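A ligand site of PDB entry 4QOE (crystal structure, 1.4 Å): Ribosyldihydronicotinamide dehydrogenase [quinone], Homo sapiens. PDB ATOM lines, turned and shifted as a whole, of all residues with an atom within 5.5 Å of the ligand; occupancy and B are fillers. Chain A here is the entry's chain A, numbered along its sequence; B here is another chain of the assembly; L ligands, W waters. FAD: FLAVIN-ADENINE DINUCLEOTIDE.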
ATOM      1  N   HIS A  12     -12.311 -18.809  21.901  1.00  0.00           N
ATOM      2  CA  HIS A  12     -11.660 -18.794  20.596  1.00  0.00           C
ATOM      3  C   HIS A  12     -12.044 -17.530  19.859  1.00  0.00           C
ATOM      4  O   HIS A  12     -13.176 -17.088  19.973  1.00  0.00           O
ATOM      5  CB  HIS A  12     -12.018 -20.047  19.769  1.00  0.00           C
ATOM      6  CG  HIS A  12     -11.057 -20.325  18.645  1.00  0.00           C
ATOM      7  ND1 HIS A  12     -10.909 -19.516  17.534  1.00  0.00           N
ATOM      8  CD2 HIS A  12     -10.150 -21.315  18.526  1.00  0.00           C
ATOM      9  CE1 HIS A  12      -9.985 -20.047  16.754  1.00  0.00           C
ATOM     10  NE2 HIS A  12      -9.519 -21.136  17.325  1.00  0.00           N
ATOM     11  N   LYS A  16     -15.576 -19.252  12.824  1.00  0.00           N
ATOM     12  CA  LYS A  16     -15.488 -20.330  11.822  1.00  0.00           C
ATOM     13  C   LYS A  16     -14.495 -21.449  12.206  1.00  0.00           C
ATOM     14  O   LYS A  16     -14.258 -22.385  11.471  1.00  0.00           O
ATOM     15  CB  LYS A  16     -15.151 -19.715  10.452  1.00  0.00           C
ATOM     16  CG  LYS A  16     -16.208 -18.743   9.934  1.00  0.00           C
ATOM     17  CD  LYS A  16     -15.858 -18.267   8.514  1.00  0.00           C
ATOM     18  CE  LYS A  16     -16.622 -16.999   8.184  1.00  0.00           C
ATOM     19  NZ  LYS A  16     -15.931 -16.225   7.094  1.00  0.00           N
ATOM     20  N   SER A  17     -13.894 -21.319  13.373  1.00  0.00           N
ATOM     21  CA  SER A  17     -12.916 -22.300  13.818  1.00  0.00           C
ATOM     22  C   SER A  17     -13.510 -23.636  14.202  1.00  0.00           C
ATOM     23  O   SER A  17     -14.731 -23.813  14.340  1.00  0.00           O
ATOM     24  CB  SER A  17     -12.160 -21.744  15.001  1.00  0.00           C
ATOM     25  OG  SER A  17     -13.011 -21.591  16.162  1.00  0.00           O
ATOM     26  N   PHE A  18     -12.619 -24.593  14.332  1.00  0.00           N
ATOM     27  CA  PHE A  18     -13.002 -25.902  14.851  1.00  0.00           C
ATOM     28  C   PHE A  18     -13.619 -25.755  16.249  1.00  0.00           C
ATOM     29  O   PHE A  18     -14.653 -26.382  16.527  1.00  0.00           O
ATOM     30  CB  PHE A  18     -11.835 -26.833  14.840  1.00  0.00           C
ATOM     31  CG  PHE A  18     -12.212 -28.269  14.984  1.00  0.00           C
ATOM     32  CD1 PHE A  18     -12.732 -28.957  13.915  1.00  0.00           C
ATOM     33  CD2 PHE A  18     -12.034 -28.938  16.161  1.00  0.00           C
ATOM     34  CE1 PHE A  18     -13.122 -30.234  14.020  1.00  0.00           C
ATOM     35  CE2 PHE A  18     -12.380 -30.273  16.253  1.00  0.00           C
ATOM     36  CZ  PHE A  18     -12.928 -30.906  15.179  1.00  0.00           C
ATOM     37  N   ASN A  19     -13.019 -24.907  17.077  1.00  0.00           N
ATOM     38  CA  ASN A  19     -13.608 -24.700  18.396  1.00  0.00           C
ATOM     39  C   ASN A  19     -15.005 -24.090  18.264  1.00  0.00           C
ATOM     40  O   ASN A  19     -15.901 -24.462  19.000  1.00  0.00           O
ATOM     41  CB  ASN A  19     -12.744 -23.749  19.226  1.00  0.00           C
ATOM     42  CG  ASN A  19     -11.725 -24.477  20.032  1.00  0.00           C
ATOM     43  OD1 ASN A  19     -11.952 -24.786  21.189  1.00  0.00           O
ATOM     44  ND2 ASN A  19     -10.606 -24.792  19.374  1.00  0.00           N
ATOM     45  N   GLY A  20     -15.165 -23.112  17.351  1.00  0.00           N
ATOM     46  CA  GLY A  20     -16.466 -22.525  17.147  1.00  0.00           C
ATOM     47  C   GLY A  20     -17.507 -23.572  16.736  1.00  0.00           C
ATOM     48  O   GLY A  20     -18.644 -23.553  17.213  1.00  0.00           O
ATOM     49  N   SER A  21     -17.108 -24.488  15.843  1.00  0.00           N
ATOM     50  CA  SER A  21     -17.955 -25.604  15.429  1.00  0.00           C
ATOM     51  C   SER A  21     -18.366 -26.483  16.635  1.00  0.00           C
ATOM     52  O   SER A  21     -19.516 -26.902  16.766  1.00  0.00           O
ATOM     53  CB  SER A  21     -17.303 -26.420  14.331  1.00  0.00           C
ATOM     54  OG  SER A  21     -17.261 -25.643  13.160  1.00  0.00           O
ATOM     55  N   PRO A 103      -9.003 -24.097  22.659  1.00  0.00           N
ATOM     56  CA  PRO A 103      -7.763 -24.672  22.151  1.00  0.00           C
ATOM     57  C   PRO A 103      -6.750 -24.703  23.290  1.00  0.00           C
ATOM     58  O   PRO A 103      -6.610 -23.754  24.049  1.00  0.00           O
ATOM     59  CB  PRO A 103      -7.362 -23.723  21.047  1.00  0.00           C
ATOM     60  CG  PRO A 103      -7.883 -22.371  21.541  1.00  0.00           C
ATOM     61  CD  PRO A 103      -9.164 -22.687  22.293  1.00  0.00           C
ATOM     62  N   LEU A 104      -5.972 -25.788  23.343  1.00  0.00           N
ATOM     63  CA  LEU A 104      -4.859 -25.950  24.240  1.00  0.00           C
ATOM     64  C   LEU A 104      -3.787 -24.907  23.878  1.00  0.00           C
ATOM     65  O   LEU A 104      -3.312 -24.876  22.744  1.00  0.00           O
ATOM     66  CB  LEU A 104      -4.295 -27.333  24.187  1.00  0.00           C
ATOM     67  CG  LEU A 104      -3.411 -27.776  25.366  1.00  0.00           C
ATOM     68  CD1 LEU A 104      -4.181 -27.874  26.652  1.00  0.00           C
ATOM     69  CD2 LEU A 104      -2.740 -29.118  25.078  1.00  0.00           C
ATOM     70  N   TYR A 105      -3.431 -24.041  24.828  1.00  0.00           N
ATOM     71  CA  TYR A 105      -2.349 -23.093  24.698  1.00  0.00           C
ATOM     72  C   TYR A 105      -1.336 -23.409  25.823  1.00  0.00           C
ATOM     73  O   TYR A 105      -1.661 -23.289  27.032  1.00  0.00           O
ATOM     74  CB  TYR A 105      -2.803 -21.630  24.871  1.00  0.00           C
ATOM     75  CG  TYR A 105      -3.445 -20.904  23.729  1.00  0.00           C
ATOM     76  CD1 TYR A 105      -3.908 -21.546  22.614  1.00  0.00           C
ATOM     77  CD2 TYR A 105      -3.595 -19.513  23.781  1.00  0.00           C
ATOM     78  CE1 TYR A 105      -4.540 -20.843  21.623  1.00  0.00           C
ATOM     79  CE2 TYR A 105      -4.168 -18.822  22.786  1.00  0.00           C
ATOM     80  CZ  TYR A 105      -4.639 -19.477  21.678  1.00  0.00           C
ATOM     81  OH  TYR A 105      -5.230 -18.740  20.698  1.00  0.00           O
ATOM     82  N   TRP A 106      -0.123 -23.836  25.426  1.00  0.00           N
ATOM     83  CA  TRP A 106       0.944 -24.147  26.375  1.00  0.00           C
ATOM     84  C   TRP A 106       0.438 -25.103  27.484  1.00  0.00           C
ATOM     85  O   TRP A 106       0.613 -24.869  28.679  1.00  0.00           O
ATOM     86  CB  TRP A 106       1.548 -22.859  26.976  1.00  0.00           C
ATOM     87  CG  TRP A 106       2.231 -22.074  25.855  1.00  0.00           C
ATOM     88  CD1 TRP A 106       2.045 -20.755  25.553  1.00  0.00           C
ATOM     89  CD2 TRP A 106       3.314 -22.513  25.040  1.00  0.00           C
ATOM     90  NE1 TRP A 106       2.867 -20.391  24.540  1.00  0.00           N
ATOM     91  CE2 TRP A 106       3.678 -21.431  24.176  1.00  0.00           C
ATOM     92  CE3 TRP A 106       4.001 -23.739  24.916  1.00  0.00           C
ATOM     93  CZ2 TRP A 106       4.702 -21.545  23.219  1.00  0.00           C
ATOM     94  CZ3 TRP A 106       5.026 -23.814  23.996  1.00  0.00           C
ATOM     95  CH2 TRP A 106       5.305 -22.761  23.125  1.00  0.00           C
ATOM     96  N   PHE A 107      -0.142 -26.216  27.016  1.00  0.00           N
ATOM     97  CA  PHE A 107      -0.552 -27.293  27.885  1.00  0.00           C
ATOM     98  C   PHE A 107      -1.582 -26.816  28.917  1.00  0.00           C
ATOM     99  O   PHE A 107      -1.777 -27.442  29.958  1.00  0.00           O
ATOM    100  CB  PHE A 107       0.650 -27.962  28.634  1.00  0.00           C
ATOM    101  CG  PHE A 107       1.421 -29.050  27.889  1.00  0.00           C
ATOM    102  CD1 PHE A 107       1.657 -28.966  26.566  1.00  0.00           C
ATOM    103  CD2 PHE A 107       1.959 -30.119  28.606  1.00  0.00           C
ATOM    104  CE1 PHE A 107       2.400 -29.943  25.885  1.00  0.00           C
ATOM    105  CE2 PHE A 107       2.745 -31.028  27.921  1.00  0.00           C
ATOM    106  CZ  PHE A 107       2.917 -30.964  26.576  1.00  0.00           C
ATOM    107  N   SER A 108      -2.317 -25.767  28.538  1.00  0.00           N
ATOM    108  CA  SER A 108      -3.281 -25.171  29.465  1.00  0.00           C
ATOM    109  C   SER A 108      -4.365 -24.413  28.675  1.00  0.00           C
ATOM    110  O   SER A 108      -4.521 -24.544  27.478  1.00  0.00           O
ATOM    111  CB  SER A 108      -2.521 -24.283  30.445  1.00  0.00           C
ATOM    112  OG  SER A 108      -3.330 -23.638  31.433  1.00  0.00           O
ATOM    113  N   THR A 148      -9.151 -28.743  22.184  1.00  0.00           N
ATOM    114  CA  THR A 148      -8.565 -29.094  20.904  1.00  0.00           C
ATOM    115  C   THR A 148      -7.050 -28.914  21.012  1.00  0.00           C
ATOM    116  O   THR A 148      -6.577 -28.048  21.743  1.00  0.00           O
ATOM    117  CB  THR A 148      -9.136 -28.206  19.777  1.00  0.00           C
ATOM    118  OG1 THR A 148      -8.757 -26.836  19.960  1.00  0.00           O
ATOM    119  CG2 THR A 148     -10.611 -28.244  19.666  1.00  0.00           C
ATOM    120  N   THR A 149      -6.261 -29.639  20.213  1.00  0.00           N
ATOM    121  CA  THR A 149      -4.830 -29.588  20.258  1.00  0.00           C
ATOM    122  C   THR A 149      -4.184 -29.430  18.902  1.00  0.00           C
ATOM    123  O   THR A 149      -4.773 -29.743  17.882  1.00  0.00           O
ATOM    124  CB  THR A 149      -4.233 -30.883  20.887  1.00  0.00           C
ATOM    125  OG1 THR A 149      -4.447 -31.936  19.968  1.00  0.00           O
ATOM    126  CG2 THR A 149      -4.850 -31.215  22.281  1.00  0.00           C
ATOM    127  N   GLY A 150      -2.942 -28.934  18.938  1.00  0.00           N
ATOM    128  CA  GLY A 150      -2.060 -29.025  17.791  1.00  0.00           C
ATOM    129  C   GLY A 150      -1.441 -30.421  17.641  1.00  0.00           C
ATOM    130  O   GLY A 150      -1.316 -30.995  16.528  1.00  0.00           O
ATOM    131  N   GLY A 151      -1.017 -30.968  18.781  1.00  0.00           N
ATOM    132  CA  GLY A 151      -0.346 -32.256  18.787  1.00  0.00           C
ATOM    133  C   GLY A 151      -1.288 -33.415  18.557  1.00  0.00           C
ATOM    134  O   GLY A 151      -2.479 -33.348  18.901  1.00  0.00           O
ATOM    135  N   TYR A 156       0.620 -37.296  22.514  1.00  0.00           N
ATOM    136  CA  TYR A 156       0.101 -37.215  23.854  1.00  0.00           C
ATOM    137  C   TYR A 156      -0.128 -38.578  24.499  1.00  0.00           C
ATOM    138  O   TYR A 156      -1.126 -38.828  25.056  1.00  0.00           O
ATOM    139  CB  TYR A 156      -1.196 -36.385  23.882  1.00  0.00           C
ATOM    140  CG  TYR A 156      -0.989 -34.904  23.763  1.00  0.00           C
ATOM    141  CD1 TYR A 156      -0.462 -34.209  24.782  1.00  0.00           C
ATOM    142  CD2 TYR A 156      -1.297 -34.253  22.625  1.00  0.00           C
ATOM    143  CE1 TYR A 156      -0.259 -32.861  24.692  1.00  0.00           C
ATOM    144  CE2 TYR A 156      -1.070 -32.905  22.518  1.00  0.00           C
ATOM    145  CZ  TYR A 156      -0.562 -32.242  23.581  1.00  0.00           C
ATOM    146  OH  TYR A 156      -0.340 -30.919  23.490  1.00  0.00           O
ATOM    147  N   ASN A 162       4.974 -35.475  24.193  1.00  0.00           N
ATOM    148  CA  ASN A 162       4.230 -34.584  25.085  1.00  0.00           C
ATOM    149  C   ASN A 162       3.817 -35.199  26.403  1.00  0.00           C
ATOM    150  O   ASN A 162       3.279 -34.519  27.251  1.00  0.00           O
ATOM    151  CB  ASN A 162       3.010 -34.023  24.388  1.00  0.00           C
ATOM    152  CG  ASN A 162       3.347 -33.075  23.285  1.00  0.00           C
ATOM    153  OD1 ASN A 162       4.407 -32.456  23.274  1.00  0.00           O
ATOM    154  ND2 ASN A 162       2.443 -32.942  22.351  1.00  0.00           N
ATOM    155  N   PRO A 193      -6.931 -31.133  14.892  1.00  0.00           N
ATOM    156  CA  PRO A 193      -7.820 -30.900  13.761  1.00  0.00           C
ATOM    157  C   PRO A 193      -7.142 -30.228  12.581  1.00  0.00           C
ATOM    158  O   PRO A 193      -7.594 -30.405  11.448  1.00  0.00           O
ATOM    159  CB  PRO A 193      -8.939 -30.037  14.371  1.00  0.00           C
ATOM    160  CG  PRO A 193      -8.290 -29.379  15.545  1.00  0.00           C
ATOM    161  CD  PRO A 193      -7.437 -30.470  16.109  1.00  0.00           C
ATOM    162  N   GLU A 194      -6.110 -29.444  12.827  1.00  0.00           N
ATOM    163  CA  GLU A 194      -5.435 -28.782  11.737  1.00  0.00           C
ATOM    164  C   GLU A 194      -4.765 -29.785  10.756  1.00  0.00           C
ATOM    165  O   GLU A 194      -4.724 -29.500   9.600  1.00  0.00           O
ATOM    166  CB  GLU A 194      -4.458 -27.739  12.270  1.00  0.00           C
ATOM    167  CG  GLU A 194      -5.140 -26.586  12.997  1.00  0.00           C
ATOM    168  CD  GLU A 194      -4.160 -25.753  13.816  1.00  0.00           C
ATOM    169  OE1 GLU A 194      -3.685 -26.214  14.822  1.00  0.00           O
ATOM    170  OE2 GLU A 194      -3.820 -24.681  13.375  1.00  0.00           O
ATOM    171  N   GLU A 198     -10.557 -33.778   6.199  1.00  0.00           N
ATOM    172  CA  GLU A 198     -11.939 -33.246   6.343  1.00  0.00           C
ATOM    173  C   GLU A 198     -12.897 -34.265   6.960  1.00  0.00           C
ATOM    174  O   GLU A 198     -13.726 -33.901   7.809  1.00  0.00           O
ATOM    175  CB  GLU A 198     -12.514 -32.774   5.008  1.00  0.00           C
ATOM    176  CG  GLU A 198     -12.621 -31.242   4.872  1.00  0.00           C
ATOM    177  CD  GLU A 198     -13.671 -30.644   5.799  1.00  0.00           C
ATOM    178  OE1 GLU A 198     -14.827 -31.137   5.815  1.00  0.00           O
ATOM    179  OE2 GLU A 198     -13.336 -29.688   6.535  1.00  0.00           O
ATOM    180  N   ARG A 201     -12.169 -34.593  10.658  1.00  0.00           N
ATOM    181  CA  ARG A 201     -12.701 -33.421  11.409  1.00  0.00           C
ATOM    182  C   ARG A 201     -14.210 -33.515  11.622  1.00  0.00           C
ATOM    183  O   ARG A 201     -14.759 -33.290  12.704  1.00  0.00           O
ATOM    184  CB  ARG A 201     -12.374 -32.160  10.649  1.00  0.00           C
ATOM    185  CG  ARG A 201     -10.882 -31.876  10.698  1.00  0.00           C
ATOM    186  CD  ARG A 201     -10.714 -30.415  10.539  1.00  0.00           C
ATOM    187  NE  ARG A 201     -10.954 -30.118   9.152  1.00  0.00           N
ATOM    188  CZ  ARG A 201      -9.977 -29.969   8.270  1.00  0.00           C
ATOM    189  NH1 ARG A 201     -10.265 -29.686   7.048  1.00  0.00           N
ATOM    190  NH2 ARG A 201      -8.697 -30.101   8.634  1.00  0.00           N
ATOM    191  N   LYS A 202     -14.878 -33.932  10.524  1.00  0.00           N
ATOM    192  CA  LYS A 202     -16.343 -34.139  10.532  1.00  0.00           C
ATOM    193  C   LYS A 202     -16.692 -35.216  11.593  1.00  0.00           C
ATOM    194  O   LYS A 202     -17.647 -35.048  12.374  1.00  0.00           O
ATOM    195  CB  LYS A 202     -16.818 -34.477   9.126  1.00  0.00           C
ATOM    196  CG  LYS A 202     -18.002 -33.673   8.665  1.00  0.00           C
ATOM    197  CD  LYS A 202     -17.651 -32.224   8.520  1.00  0.00           C
ATOM    198  CE  LYS A 202     -18.622 -31.579   7.554  1.00  0.00           C
ATOM    199  NZ  LYS A 202     -18.505 -30.095   7.617  1.00  0.00           N
ATOM    200  N   VAL A 205     -16.342 -33.802  15.202  1.00  0.00           N
ATOM    201  CA  VAL A 205     -17.486 -32.946  15.501  1.00  0.00           C
ATOM    202  C   VAL A 205     -18.718 -33.840  15.823  1.00  0.00           C
ATOM    203  O   VAL A 205     -19.404 -33.644  16.830  1.00  0.00           O
ATOM    204  CB  VAL A 205     -17.786 -31.911  14.383  1.00  0.00           C
ATOM    205  CG1 VAL A 205     -19.032 -31.102  14.681  1.00  0.00           C
ATOM    206  CG2 VAL A 205     -16.621 -30.948  14.185  1.00  0.00           C
ATOM    207  N   ASN B  67      -6.513 -17.300  12.385  1.00  0.00           N
ATOM    208  CA  ASN B  67      -5.797 -18.365  13.056  1.00  0.00           C
ATOM    209  C   ASN B  67      -4.643 -17.719  13.798  1.00  0.00           C
ATOM    210  O   ASN B  67      -3.688 -17.320  13.207  1.00  0.00           O
ATOM    211  CB  ASN B  67      -5.274 -19.383  12.031  1.00  0.00           C
ATOM    212  CG  ASN B  67      -4.615 -20.570  12.655  1.00  0.00           C
ATOM    213  OD1 ASN B  67      -3.785 -20.497  13.508  1.00  0.00           O
ATOM    214  ND2 ASN B  67      -4.994 -21.728  12.167  1.00  0.00           N
ATOM    215  N   TYR B  68      -4.738 -17.615  15.119  1.00  0.00           N
ATOM    216  CA  TYR B  68      -3.788 -16.805  15.857  1.00  0.00           C
ATOM    217  C   TYR B  68      -2.376 -17.350  15.634  1.00  0.00           C
ATOM    218  O   TYR B  68      -1.436 -16.571  15.416  1.00  0.00           O
ATOM    219  CB  TYR B  68      -4.119 -16.804  17.364  1.00  0.00           C
ATOM    220  CG  TYR B  68      -3.221 -15.914  18.179  1.00  0.00           C
ATOM    221  CD1 TYR B  68      -3.413 -14.508  18.146  1.00  0.00           C
ATOM    222  CD2 TYR B  68      -2.109 -16.411  18.820  1.00  0.00           C
ATOM    223  CE1 TYR B  68      -2.568 -13.659  18.866  1.00  0.00           C
ATOM    224  CE2 TYR B  68      -1.249 -15.565  19.521  1.00  0.00           C
ATOM    225  CZ  TYR B  68      -1.498 -14.205  19.534  1.00  0.00           C
ATOM    226  OH  TYR B  68      -0.640 -13.368  20.203  1.00  0.00           O
ATOM    227  N   GLY B  69      -2.206 -18.652  15.711  1.00  0.00           N
ATOM    228  CA  GLY B  69      -0.847 -19.232  15.546  1.00  0.00           C
ATOM    229  C   GLY B  69      -0.221 -18.987  14.201  1.00  0.00           C
ATOM    230  O   GLY B  69       0.962 -18.626  14.106  1.00  0.00           O
ATOM    231  N   ASP B 118       1.725 -16.961  26.086  1.00  0.00           N
ATOM    232  CA  ASP B 118       0.933 -17.196  24.866  1.00  0.00           C
ATOM    233  C   ASP B 118       1.385 -16.276  23.714  1.00  0.00           C
ATOM    234  O   ASP B 118       1.430 -16.681  22.554  1.00  0.00           O
ATOM    235  CB  ASP B 118      -0.561 -16.920  25.149  1.00  0.00           C
ATOM    236  CG  ASP B 118      -1.220 -17.901  26.090  1.00  0.00           C
ATOM    237  OD1 ASP B 118      -0.629 -18.943  26.430  1.00  0.00           O
ATOM    238  OD2 ASP B 118      -2.362 -17.555  26.484  1.00  0.00           O
ATOM    239  N   GLY B 175       5.807 -28.440  29.037  1.00  0.00           N
ATOM    240  CA  GLY B 175       4.996 -28.070  27.878  1.00  0.00           C
ATOM    241  C   GLY B 175       5.312 -26.684  27.299  1.00  0.00           C
ATOM    242  O   GLY B 175       5.033 -26.436  26.144  1.00  0.00           O
HETATM  243  PA  FAD L   1      -8.940 -24.483  13.322  1.00  0.00           P
HETATM  244  O1A FAD L   1      -9.954 -23.462  13.389  1.00  0.00           O
HETATM  245  O2A FAD L   1      -7.674 -24.094  12.640  1.00  0.00           O
HETATM  246  O5B FAD L   1      -9.595 -25.668  12.587  1.00  0.00           O
HETATM  247  C5B FAD L   1      -8.921 -26.717  11.946  1.00  0.00           C
HETATM  248  C4B FAD L   1      -9.678 -26.889  10.659  1.00  0.00           C
HETATM  249  O4B FAD L   1     -11.033 -27.358  10.887  1.00  0.00           O
HETATM  250  C3B FAD L   1      -9.815 -25.616   9.846  1.00  0.00           C
HETATM  251  O3B FAD L   1      -9.498 -26.003   8.523  1.00  0.00           O
HETATM  252  C2B FAD L   1     -11.297 -25.255   9.970  1.00  0.00           C
HETATM  253  O2B FAD L   1     -11.807 -24.598   8.816  1.00  0.00           O
HETATM  254  C1B FAD L   1     -11.889 -26.642  10.040  1.00  0.00           C
HETATM  255  N9A FAD L   1     -13.247 -26.766  10.525  1.00  0.00           N
HETATM  256  C8A FAD L   1     -13.939 -25.892  11.340  1.00  0.00           C
HETATM  257  N7A FAD L   1     -15.170 -26.265  11.590  1.00  0.00           N
HETATM  258  C5A FAD L   1     -15.285 -27.484  10.945  1.00  0.00           C
HETATM  259  C6A FAD L   1     -16.319 -28.439  10.898  1.00  0.00           C
HETATM  260  N6A FAD L   1     -17.502 -28.251  11.435  1.00  0.00           N
HETATM  261  N1A FAD L   1     -16.087 -29.584  10.211  1.00  0.00           N
HETATM  262  C2A FAD L   1     -14.919 -29.747   9.594  1.00  0.00           C
HETATM  263  N3A FAD L   1     -13.860 -28.926   9.573  1.00  0.00           N
HETATM  264  C4A FAD L   1     -14.110 -27.799  10.275  1.00  0.00           C
HETATM  265  N1  FAD L   1      -1.157 -27.341  20.784  1.00  0.00           N
HETATM  266  C2  FAD L   1      -0.785 -28.318  21.594  1.00  0.00           C
HETATM  267  O2  FAD L   1      -0.966 -29.545  21.307  1.00  0.00           O
HETATM  268  N3  FAD L   1      -0.151 -28.013  22.731  1.00  0.00           N
HETATM  269  C4  FAD L   1       0.176 -26.731  23.170  1.00  0.00           C
HETATM  270  O4  FAD L   1       0.722 -26.610  24.246  1.00  0.00           O
HETATM  271  C4X FAD L   1      -0.150 -25.718  22.280  1.00  0.00           C
HETATM  272  N5  FAD L   1       0.182 -24.454  22.614  1.00  0.00           N
HETATM  273  C5X FAD L   1      -0.296 -23.450  21.804  1.00  0.00           C
HETATM  274  C6  FAD L   1      -0.042 -22.119  22.148  1.00  0.00           C
HETATM  275  C7  FAD L   1      -0.540 -21.072  21.372  1.00  0.00           C
HETATM  276  C7M FAD L   1      -0.337 -19.641  21.806  1.00  0.00           C
HETATM  277  C8  FAD L   1      -1.253 -21.368  20.184  1.00  0.00           C
HETATM  278  C8M FAD L   1      -1.771 -20.282  19.279  1.00  0.00           C
HETATM  279  C9  FAD L   1      -1.485 -22.702  19.843  1.00  0.00           C
HETATM  280  C9A FAD L   1      -1.050 -23.730  20.634  1.00  0.00           C
HETATM  281  N10 FAD L   1      -1.290 -25.079  20.309  1.00  0.00           N
HETATM  282  C10 FAD L   1      -0.849 -26.076  21.126  1.00  0.00           C
HETATM  283  C1' FAD L   1      -2.071 -25.418  19.105  1.00  0.00           C
HETATM  284  C2' FAD L   1      -3.575 -25.157  19.292  1.00  0.00           C
HETATM  285  O2' FAD L   1      -4.048 -25.989  20.353  1.00  0.00           O
HETATM  286  C3' FAD L   1      -4.324 -25.596  18.036  1.00  0.00           C
HETATM  287  O3' FAD L   1      -3.903 -24.690  17.010  1.00  0.00           O
HETATM  288  C4' FAD L   1      -5.848 -25.527  18.160  1.00  0.00           C
HETATM  289  O4' FAD L   1      -6.281 -26.477  19.158  1.00  0.00           O
HETATM  290  C5' FAD L   1      -6.580 -25.809  16.880  1.00  0.00           C
HETATM  291  O5' FAD L   1      -7.960 -25.574  17.029  1.00  0.00           O
HETATM  292  P   FAD L   1      -8.713 -24.486  16.224  1.00  0.00           P
HETATM  293  O1P FAD L   1     -10.132 -24.402  16.559  1.00  0.00           O
HETATM  294  O2P FAD L   1      -7.952 -23.236  16.299  1.00  0.00           O
HETATM  295  O3P FAD L   1      -8.540 -25.139  14.717  1.00  0.00           O
HETATM  296  O   HOH W   1     -12.256 -22.369   9.711  1.00  0.00           O
HETATM  297  O   HOH W   2     -19.805 -30.204  11.075  1.00  0.00           O
HETATM  298  O   HOH W   3      -6.154 -21.915  18.043  1.00  0.00           O
HETATM  299  O   HOH W   4     -10.232 -21.641  11.466  1.00  0.00           O
HETATM  300  O   HOH W   5       2.752 -18.851  21.586  1.00  0.00           O
HETATM  301  O   HOH W   6      -7.273 -21.108  14.549  1.00  0.00           O
HETATM  302  O   HOH W   7      -9.322 -20.166  13.335  1.00  0.00           O
HETATM  303  O   HOH W   8      -6.677 -23.689  10.309  1.00  0.00           O
HETATM  304  O   HOH W   9       3.512 -27.193  23.822  1.00  0.00           O
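O2 of the ligand is in hydrogen-bond range of N of Gly 151 (2.9 Å).
The backbone carbonyl oxygen (O) of Thr 148 sits at hydrogen-bond distance from an oxygen (O4') of the ligand, at 3.0 Å.
ND2 of Asn 19 sits at hydrogen-bond distance from O1P of the ligand.
O3' of the ligand lies within hydrogen-bond range of OE1 of Glu 194 (2.7 Å).
N of Thr 149 sits at hydrogen-bond distance from O4' of the ligand.
A ring nitrogen (NE2) of His 12 is in hydrogen-bond range of an oxygen (O2P) of the ligand, 2.8 Å away.
N of Gly 150 sits at hydrogen-bond distance from N1 of the ligand (3.0 Å).
The side-chain hydroxyl of Tyr 156 lies within hydrogen-bond range of an oxygen (O2) of the ligand.
The side-chain hydroxyl (OG1) of Thr 148 lies within hydrogen-bond range of an oxygen (O4') of the ligand, 2.6 Å away.
An oxygen (O1P) of the ligand sits at hydrogen-bond distance from the backbone NH of Asn 19, 3.0 Å away.
The backbone NH (N) of Phe 18 is in hydrogen-bond range of an oxygen (O1A) of the ligand, 3.0 Å away.
N of Trp 106 lies within hydrogen-bond range of N5 of the ligand, at 2.9 Å.
O of Leu 104 is in hydrogen-bond range of O2' of the ligand (2.7 Å).
OG of Ser 21 is in hydrogen-bond range of N7A of the ligand (2.7 Å).
An oxygen (O4) of the ligand sits at hydrogen-bond distance from the backbone NH of Phe 107, 2.9 Å away.
A nitrogen (N3A) of the ligand sits at hydrogen-bond distance from the guanidinium group (NE) of Arg 201.
The guanidinium group (NH1) of Arg 201 lies within salt-bridge range of the side-chain carboxylate (OE2) of Glu 198, at 3.1 Å.
OD1 of Asn 67 of chain B lies close to N of Gly 69 of chain B, at 3.3 Å.
The side-chain hydroxyl of Thr 148 lies within hydrogen-bond range of the side-chain amide nitrogen of Asn 19 (2.8 Å).
The side-chain hydroxyl (OG) of Ser 17 sits close to the backbone NH (N) of Asn 19, 3.4 Å away.
O of Pro 193 sits at hydrogen-bond distance from NH2 of Arg 201 (3.0 Å).
O of Thr 148 sits at hydrogen-bond distance from N of Leu 104 (2.8 Å).
The backbone carbonyl oxygen (O) of Ser 17 is in hydrogen-bond range of the side-chain hydroxyl (OG) of Ser 21 (3.3 Å).
A ring nitrogen (ND1) of His 12 lies within hydrogen-bond range of the side-chain hydroxyl (OG) of Ser 17 (3.3 Å).
A nitrogen (N3A) of the ligand sits close to the side-chain carboxylate of Glu 198 (3.2 Å).
Residues that only touch the ligand: Ser 17 (3.2 Å), Lys 202 (3.5 Å), Pro 103 (3.5 Å), Lys 16 (3.5 Å), Asp 118 of chain B (3.5 Å), Tyr 105 (3.5 Å), Asn 67 of chain B (3.6 Å), Tyr 68 of chain B (3.9 Å), Gly 69 of chain B (3.9 Å), Pro 193 (3.95 Å) and Val 205 (3.95 Å).
Hydrophobic or aromatic side chains that line the ligand: His 12, Phe 18, Pro 103, Leu 104, Tyr 105, Phe 107, Tyr 156, Val 205 and Tyr 68 of chain B.
26 residues have an atom within 4 Å of the ligand: His 12, Lys 16, Ser 17, Phe 18, Asn 19, Ser 21, Pro 103, Leu 104, Tyr 105, Trp 106, Phe 107, Thr 148, Thr 149, Gly 150, Gly 151, Tyr 156, Pro 193, Glu 194, Glu 198, Arg 201, Lys 202, Val 205, Asn 67 of chain B, Tyr 68 of chain B, Gly 69 of chain B and Asp 118 of chain B.
Water W1 lies within hydrogen-bond range of O2B of the ligand (2.4 Å) and O of Lys 16 (2.7 Å).
Water W8 bridges an oxygen (O2A) of the ligand and the side-chain amide nitrogen of Asn 67 of chain B.
Water W6 lies within hydrogen-bond range of O2P of the ligand (2.8 Å) and ND2 of Asn 67 of chain B (3.4 Å).
Water W9 bridges O of Gly 175 of chain B (2.9 Å) and O4 of the ligand (2.9 Å).
Water W5 lies within hydrogen-bond range of O of Asp 118 of chain B and NE1 of Trp 106.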
